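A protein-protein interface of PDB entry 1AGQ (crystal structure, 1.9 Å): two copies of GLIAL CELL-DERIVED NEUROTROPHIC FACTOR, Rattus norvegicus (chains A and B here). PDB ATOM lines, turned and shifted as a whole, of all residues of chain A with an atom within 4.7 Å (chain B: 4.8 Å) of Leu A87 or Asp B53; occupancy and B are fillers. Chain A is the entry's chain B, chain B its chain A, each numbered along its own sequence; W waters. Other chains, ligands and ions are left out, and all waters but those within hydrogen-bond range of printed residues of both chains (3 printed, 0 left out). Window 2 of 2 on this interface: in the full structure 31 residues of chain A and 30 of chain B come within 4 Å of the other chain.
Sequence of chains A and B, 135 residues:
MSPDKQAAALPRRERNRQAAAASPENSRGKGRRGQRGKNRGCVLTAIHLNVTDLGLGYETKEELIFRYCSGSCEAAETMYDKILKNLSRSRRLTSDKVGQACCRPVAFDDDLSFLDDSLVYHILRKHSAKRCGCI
The guanidinium group (NH1) of Arg A92 is in salt-bridge range of the side-chain carboxylate (OD1) of Asp B53 (3.7 Å). O of Leu B54 is in hydrogen-bond range of ND2 of Asn A86. ND2 of Asn A86 lies within hydrogen-bond range of O of Gly B55 (3.3 Å).
Leu A87 touches three residues of chain B. Of chain A, only Leu A87 and Arg A92 come within 4 Å of Asp B53. Printed residues of chain B within 4 Å of Leu A84: Phe B66. Printed residues of chain B within 4 Å of Ile A83: Leu B54 and Phe B66. Of the printed residues of chain A, Gly B55 touches Asn A86. Of the printed residues of chain B, Arg A92 touches Leu B49 (3.7 Å) and Asp B53 (3.7 Å). Lys A85 touches none of the printed residues of chain B. The nearest printed residue of chain B that does not touch Leu A87 is Leu B54 (4.9 Å). The nearest printed residue of chain A that does not touch Asp B53 is Ser A90 (4.9 Å).
Of the 11 printed residues of chain A, 5 touch a printed residue of chain B. Hydrophobic or aromatic side chains of chain B that line the printed part of chain A: Leu B49, Leu B54 and Phe B66. Among the printed residues, Asp or Glu carboxylates within 4 Å of a Lys or Arg side-chain nitrogen of the other chain: Arg A92 with Asp B53 (3.7 Å).
Among the printed residues, merely in contact across the chains: Leu A87 with Asp B53, Leu A87 with Phe B66, Ile A83 with Phe B66, Arg A92 with Leu B49, Ile A83 with Leu B54, Leu A87 with Leu B49 and Leu A84 with Phe B66.
Water W2 bridges the side-chain hydroxyl of Ser A90 (2.6 Å) and the backbone carbonyl oxygen of Asp B53 (2.8 Å). Water W3 lies within hydrogen-bond range of NH1 of Arg A92, OD2 of Asp B53 and ND2 of Asn B50. Water W1 bridges the side-chain amide nitrogen (ND2) of Asn A86 and the backbone carbonyl oxygen (O) of Gly B55.
No position is printed for both chains. Of the 10 pairs that touch across the chains among the printed residues, none has its exchanged pair printed and touching as well.
The backbone NH (N) of Asn B50 is in hydrogen-bond range of the side-chain carboxylate (OD2) of Asp B53, at 2.8 Å. The backbone carbonyl oxygen (O) of Asn A86 sits at hydrogen-bond distance from the side-chain hydroxyl (OG) of Ser A90, 3.2 Å away. The backbone carbonyl oxygen (O) of Leu A87 is in hydrogen-bond range of the side-chain hydroxyl (OG) of Ser A90. O of Leu A87 sits at hydrogen-bond distance from N of Arg A92. The backbone NH (N) of Leu A93 sits at hydrogen-bond distance from the backbone carbonyl oxygen (O) of Leu A87, 3.2 Å away.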
ATOM      1  N   ILE A  83      -7.209  19.681 -19.389  1.00  0.00           N
ATOM      2  CA  ILE A  83      -6.950  20.633 -20.459  1.00  0.00           C
ATOM      3  C   ILE A  83      -7.061  22.065 -19.952  1.00  0.00           C
ATOM      4  O   ILE A  83      -6.211  22.898 -20.235  1.00  0.00           O
ATOM      5  CB  ILE A  83      -7.912  20.384 -21.634  1.00  0.00           C
ATOM      6  CG1 ILE A  83      -7.538  19.052 -22.301  1.00  0.00           C
ATOM      7  CG2 ILE A  83      -7.827  21.562 -22.668  1.00  0.00           C
ATOM      8  CD1 ILE A  83      -8.459  18.651 -23.422  1.00  0.00           C
ATOM      9  N   LEU A  84      -8.101  22.358 -19.174  1.00  0.00           N
ATOM     10  CA  LEU A  84      -8.257  23.694 -18.600  1.00  0.00           C
ATOM     11  C   LEU A  84      -7.056  24.112 -17.747  1.00  0.00           C
ATOM     12  O   LEU A  84      -6.594  25.257 -17.814  1.00  0.00           O
ATOM     13  CB  LEU A  84      -9.550  23.735 -17.750  1.00  0.00           C
ATOM     14  CG  LEU A  84     -10.868  23.844 -18.516  1.00  0.00           C
ATOM     15  CD1 LEU A  84     -12.018  24.061 -17.535  1.00  0.00           C
ATOM     16  CD2 LEU A  84     -10.815  25.001 -19.498  1.00  0.00           C
ATOM     17  N   LYS A  85      -6.547  23.178 -16.949  1.00  0.00           N
ATOM     18  CA  LYS A  85      -5.415  23.426 -16.083  1.00  0.00           C
ATOM     19  C   LYS A  85      -4.235  23.742 -16.979  1.00  0.00           C
ATOM     20  O   LYS A  85      -3.476  24.674 -16.720  1.00  0.00           O
ATOM     21  CB  LYS A  85      -5.099  22.179 -15.255  1.00  0.00           C
ATOM     22  CG  LYS A  85      -5.097  22.378 -13.745  1.00  0.00           C
ATOM     23  CD  LYS A  85      -5.289  21.040 -13.023  1.00  0.00           C
ATOM     24  CE  LYS A  85      -6.470  21.088 -12.050  1.00  0.00           C
ATOM     25  NZ  LYS A  85      -7.735  20.529 -12.628  1.00  0.00           N
ATOM     26  N   ASN A  86      -4.094  22.974 -18.059  1.00  0.00           N
ATOM     27  CA  ASN A  86      -2.956  23.205 -18.967  1.00  0.00           C
ATOM     28  C   ASN A  86      -3.063  24.545 -19.731  1.00  0.00           C
ATOM     29  O   ASN A  86      -2.059  25.244 -19.923  1.00  0.00           O
ATOM     30  CB  ASN A  86      -2.835  22.036 -19.953  1.00  0.00           C
ATOM     31  CG  ASN A  86      -2.485  20.710 -19.259  1.00  0.00           C
ATOM     32  OD1 ASN A  86      -1.982  20.693 -18.139  1.00  0.00           O
ATOM     33  ND2 ASN A  86      -2.758  19.595 -19.937  1.00  0.00           N
ATOM     34  N   LEU A  87      -4.258  24.893 -20.177  1.00  0.00           N
ATOM     35  CA  LEU A  87      -4.425  26.153 -20.918  1.00  0.00           C
ATOM     36  C   LEU A  87      -4.247  27.344 -20.021  1.00  0.00           C
ATOM     37  O   LEU A  87      -3.850  28.437 -20.470  1.00  0.00           O
ATOM     38  CB  LEU A  87      -5.793  26.195 -21.594  1.00  0.00           C
ATOM     39  CG  LEU A  87      -5.962  25.100 -22.650  1.00  0.00           C
ATOM     40  CD1 LEU A  87      -7.389  25.156 -23.213  1.00  0.00           C
ATOM     41  CD2 LEU A  87      -4.912  25.267 -23.772  1.00  0.00           C
ATOM     42  N   SER A  88      -4.529  27.163 -18.732  1.00  0.00           N
ATOM     43  CA  SER A  88      -4.352  28.278 -17.800  1.00  0.00           C
ATOM     44  C   SER A  88      -2.858  28.485 -17.566  1.00  0.00           C
ATOM     45  O   SER A  88      -2.355  29.619 -17.551  1.00  0.00           O
ATOM     46  CB  SER A  88      -5.088  27.977 -16.469  1.00  0.00           C
ATOM     47  OG  SER A  88      -4.743  28.936 -15.486  1.00  0.00           O
ATOM     48  N   ARG A  89      -2.119  27.380 -17.416  1.00  0.00           N
ATOM     49  CA  ARG A  89      -0.688  27.491 -17.197  1.00  0.00           C
ATOM     50  C   ARG A  89      -0.012  28.101 -18.411  1.00  0.00           C
ATOM     51  O   ARG A  89       0.963  28.838 -18.255  1.00  0.00           O
ATOM     52  CB  ARG A  89      -0.030  26.120 -16.927  1.00  0.00           C
ATOM     53  N   SER A  90      -0.520  27.795 -19.606  1.00  0.00           N
ATOM     54  CA  SER A  90       0.086  28.305 -20.851  1.00  0.00           C
ATOM     55  C   SER A  90      -0.387  29.697 -21.233  1.00  0.00           C
ATOM     56  O   SER A  90       0.081  30.277 -22.221  1.00  0.00           O
ATOM     57  CB  SER A  90      -0.181  27.336 -22.015  1.00  0.00           C
ATOM     58  OG  SER A  90      -1.546  27.298 -22.388  1.00  0.00           O
ATOM     59  N   ARG A  91      -1.331  30.221 -20.461  1.00  0.00           N
ATOM     60  CA  ARG A  91      -1.882  31.552 -20.675  1.00  0.00           C
ATOM     61  C   ARG A  91      -2.727  31.668 -21.942  1.00  0.00           C
ATOM     62  O   ARG A  91      -2.876  32.747 -22.486  1.00  0.00           O
ATOM     63  CB  ARG A  91      -0.749  32.605 -20.697  1.00  0.00           C
ATOM     64  CG  ARG A  91       0.140  32.688 -19.423  1.00  0.00           C
ATOM     65  CD  ARG A  91      -0.637  32.557 -18.113  1.00  0.00           C
ATOM     66  NE  ARG A  91       0.120  33.053 -16.958  1.00  0.00           N
ATOM     67  CZ  ARG A  91       0.528  32.301 -15.937  1.00  0.00           C
ATOM     68  NH1 ARG A  91       0.270  31.008 -15.899  1.00  0.00           N
ATOM     69  NH2 ARG A  91       1.219  32.873 -14.932  1.00  0.00           N
ATOM     70  N   ARG A  92      -3.291  30.555 -22.419  1.00  0.00           N
ATOM     71  CA  ARG A  92      -4.135  30.598 -23.593  1.00  0.00           C
ATOM     72  C   ARG A  92      -5.590  30.724 -23.179  1.00  0.00           C
ATOM     73  O   ARG A  92      -6.464  31.020 -23.990  1.00  0.00           O
ATOM     74  CB  ARG A  92      -3.953  29.358 -24.459  1.00  0.00           C
ATOM     75  CG  ARG A  92      -2.531  29.238 -24.988  1.00  0.00           C
ATOM     76  CD  ARG A  92      -2.245  30.285 -26.069  1.00  0.00           C
ATOM     77  NE  ARG A  92      -3.191  30.294 -27.192  1.00  0.00           N
ATOM     78  CZ  ARG A  92      -3.032  29.626 -28.333  1.00  0.00           C
ATOM     79  NH1 ARG A  92      -1.925  28.878 -28.494  1.00  0.00           N
ATOM     80  NH2 ARG A  92      -3.911  29.696 -29.292  1.00  0.00           N
ATOM     81  N   LEU A  93      -5.822  30.496 -21.890  1.00  0.00           N
ATOM     82  CA  LEU A  93      -7.151  30.579 -21.292  1.00  0.00           C
ATOM     83  C   LEU A  93      -6.961  30.692 -19.777  1.00  0.00           C
ATOM     84  O   LEU A  93      -6.815  29.669 -19.108  1.00  0.00           O
ATOM     85  CB  LEU A  93      -7.936  29.306 -21.610  1.00  0.00           C
ATOM     86  CG  LEU A  93      -9.341  29.231 -21.052  1.00  0.00           C
ATOM     87  CD1 LEU A  93     -10.092  30.476 -21.470  1.00  0.00           C
ATOM     88  CD2 LEU A  93     -10.022  27.973 -21.559  1.00  0.00           C
ATOM     89  N   LEU B  49      -7.345  25.401 -31.460  1.00  0.00           N
ATOM     90  CA  LEU B  49      -6.054  25.020 -30.912  1.00  0.00           C
ATOM     91  C   LEU B  49      -5.465  23.845 -31.719  1.00  0.00           C
ATOM     92  O   LEU B  49      -6.167  23.175 -32.486  1.00  0.00           O
ATOM     93  CB  LEU B  49      -6.204  24.532 -29.463  1.00  0.00           C
ATOM     94  CG  LEU B  49      -6.742  25.493 -28.391  1.00  0.00           C
ATOM     95  CD1 LEU B  49      -6.985  24.724 -27.064  1.00  0.00           C
ATOM     96  CD2 LEU B  49      -5.743  26.610 -28.211  1.00  0.00           C
ATOM     97  N   ASN B  50      -4.192  23.611 -31.496  1.00  0.00           N
ATOM     98  CA  ASN B  50      -3.508  22.453 -32.064  1.00  0.00           C
ATOM     99  C   ASN B  50      -3.627  21.405 -30.939  1.00  0.00           C
ATOM    100  O   ASN B  50      -3.719  21.768 -29.777  1.00  0.00           O
ATOM    101  CB  ASN B  50      -2.044  22.781 -32.279  1.00  0.00           C
ATOM    102  CG  ASN B  50      -1.860  23.919 -33.263  1.00  0.00           C
ATOM    103  OD1 ASN B  50      -2.550  23.972 -34.267  1.00  0.00           O
ATOM    104  ND2 ASN B  50      -0.966  24.850 -32.944  1.00  0.00           N
ATOM    105  N   VAL B  51      -3.619  20.115 -31.252  1.00  0.00           N
ATOM    106  CA  VAL B  51      -3.683  19.141 -30.179  1.00  0.00           C
ATOM    107  C   VAL B  51      -2.486  19.346 -29.240  1.00  0.00           C
ATOM    108  O   VAL B  51      -2.564  19.121 -28.022  1.00  0.00           O
ATOM    109  CB  VAL B  51      -3.706  17.707 -30.752  1.00  0.00           C
ATOM    110  CG1 VAL B  51      -3.279  16.716 -29.673  1.00  0.00           C
ATOM    111  CG2 VAL B  51      -5.095  17.387 -31.228  1.00  0.00           C
ATOM    112  N   THR B  52      -1.368  19.818 -29.785  1.00  0.00           N
ATOM    113  CA  THR B  52      -0.192  20.055 -28.965  1.00  0.00           C
ATOM    114  C   THR B  52      -0.403  21.161 -27.907  1.00  0.00           C
ATOM    115  O   THR B  52       0.371  21.278 -26.956  1.00  0.00           O
ATOM    116  CB  THR B  52       1.017  20.437 -29.829  1.00  0.00           C
ATOM    117  OG1 THR B  52       0.671  21.540 -30.679  1.00  0.00           O
ATOM    118  CG2 THR B  52       1.451  19.245 -30.697  1.00  0.00           C
ATOM    119  N   ASP B  53      -1.441  21.972 -28.070  1.00  0.00           N
ATOM    120  CA  ASP B  53      -1.717  23.047 -27.100  1.00  0.00           C
ATOM    121  C   ASP B  53      -2.425  22.491 -25.869  1.00  0.00           C
ATOM    122  O   ASP B  53      -2.475  23.148 -24.842  1.00  0.00           O
ATOM    123  CB  ASP B  53      -2.629  24.115 -27.706  1.00  0.00           C
ATOM    124  CG  ASP B  53      -1.940  24.935 -28.767  1.00  0.00           C
ATOM    125  OD1 ASP B  53      -0.787  25.342 -28.534  1.00  0.00           O
ATOM    126  OD2 ASP B  53      -2.570  25.185 -29.820  1.00  0.00           O
ATOM    127  N   LEU B  54      -2.991  21.293 -25.985  1.00  0.00           N
ATOM    128  CA  LEU B  54      -3.722  20.675 -24.880  1.00  0.00           C
ATOM    129  C   LEU B  54      -2.844  20.288 -23.684  1.00  0.00           C
ATOM    130  O   LEU B  54      -3.359  20.051 -22.576  1.00  0.00           O
ATOM    131  CB  LEU B  54      -4.487  19.471 -25.412  1.00  0.00           C
ATOM    132  CG  LEU B  54      -5.373  19.865 -26.598  1.00  0.00           C
ATOM    133  CD1 LEU B  54      -6.091  18.644 -27.121  1.00  0.00           C
ATOM    134  CD2 LEU B  54      -6.404  20.917 -26.140  1.00  0.00           C
ATOM    135  N   GLY B  55      -1.530  20.256 -23.908  1.00  0.00           N
ATOM    136  CA  GLY B  55      -0.555  19.938 -22.876  1.00  0.00           C
ATOM    137  C   GLY B  55      -0.570  18.470 -22.451  1.00  0.00           C
ATOM    138  O   GLY B  55      -0.151  18.136 -21.336  1.00  0.00           O
ATOM    139  N   PHE B  66     -11.575  23.673 -29.506  1.00  0.00           N
ATOM    140  CA  PHE B  66     -11.808  23.324 -28.101  1.00  0.00           C
ATOM    141  C   PHE B  66     -12.883  24.278 -27.587  1.00  0.00           C
ATOM    142  O   PHE B  66     -12.774  25.487 -27.781  1.00  0.00           O
ATOM    143  CB  PHE B  66     -10.549  23.520 -27.277  1.00  0.00           C
ATOM    144  CG  PHE B  66     -10.756  23.361 -25.780  1.00  0.00           C
ATOM    145  CD1 PHE B  66     -11.079  22.120 -25.216  1.00  0.00           C
ATOM    146  CD2 PHE B  66     -10.598  24.463 -24.934  1.00  0.00           C
ATOM    147  CE1 PHE B  66     -11.239  21.988 -23.815  1.00  0.00           C
ATOM    148  CE2 PHE B  66     -10.756  24.348 -23.549  1.00  0.00           C
ATOM    149  CZ  PHE B  66     -11.079  23.096 -22.987  1.00  0.00           C
HETATM  150  O   HOH W   1      -1.758  17.193 -18.535  1.00  0.00           O
HETATM  151  O   HOH W   2      -1.537  25.720 -24.415  1.00  0.00           O
HETATM  152  O   HOH W   3      -1.490  27.537 -30.889  1.00  0.00           O
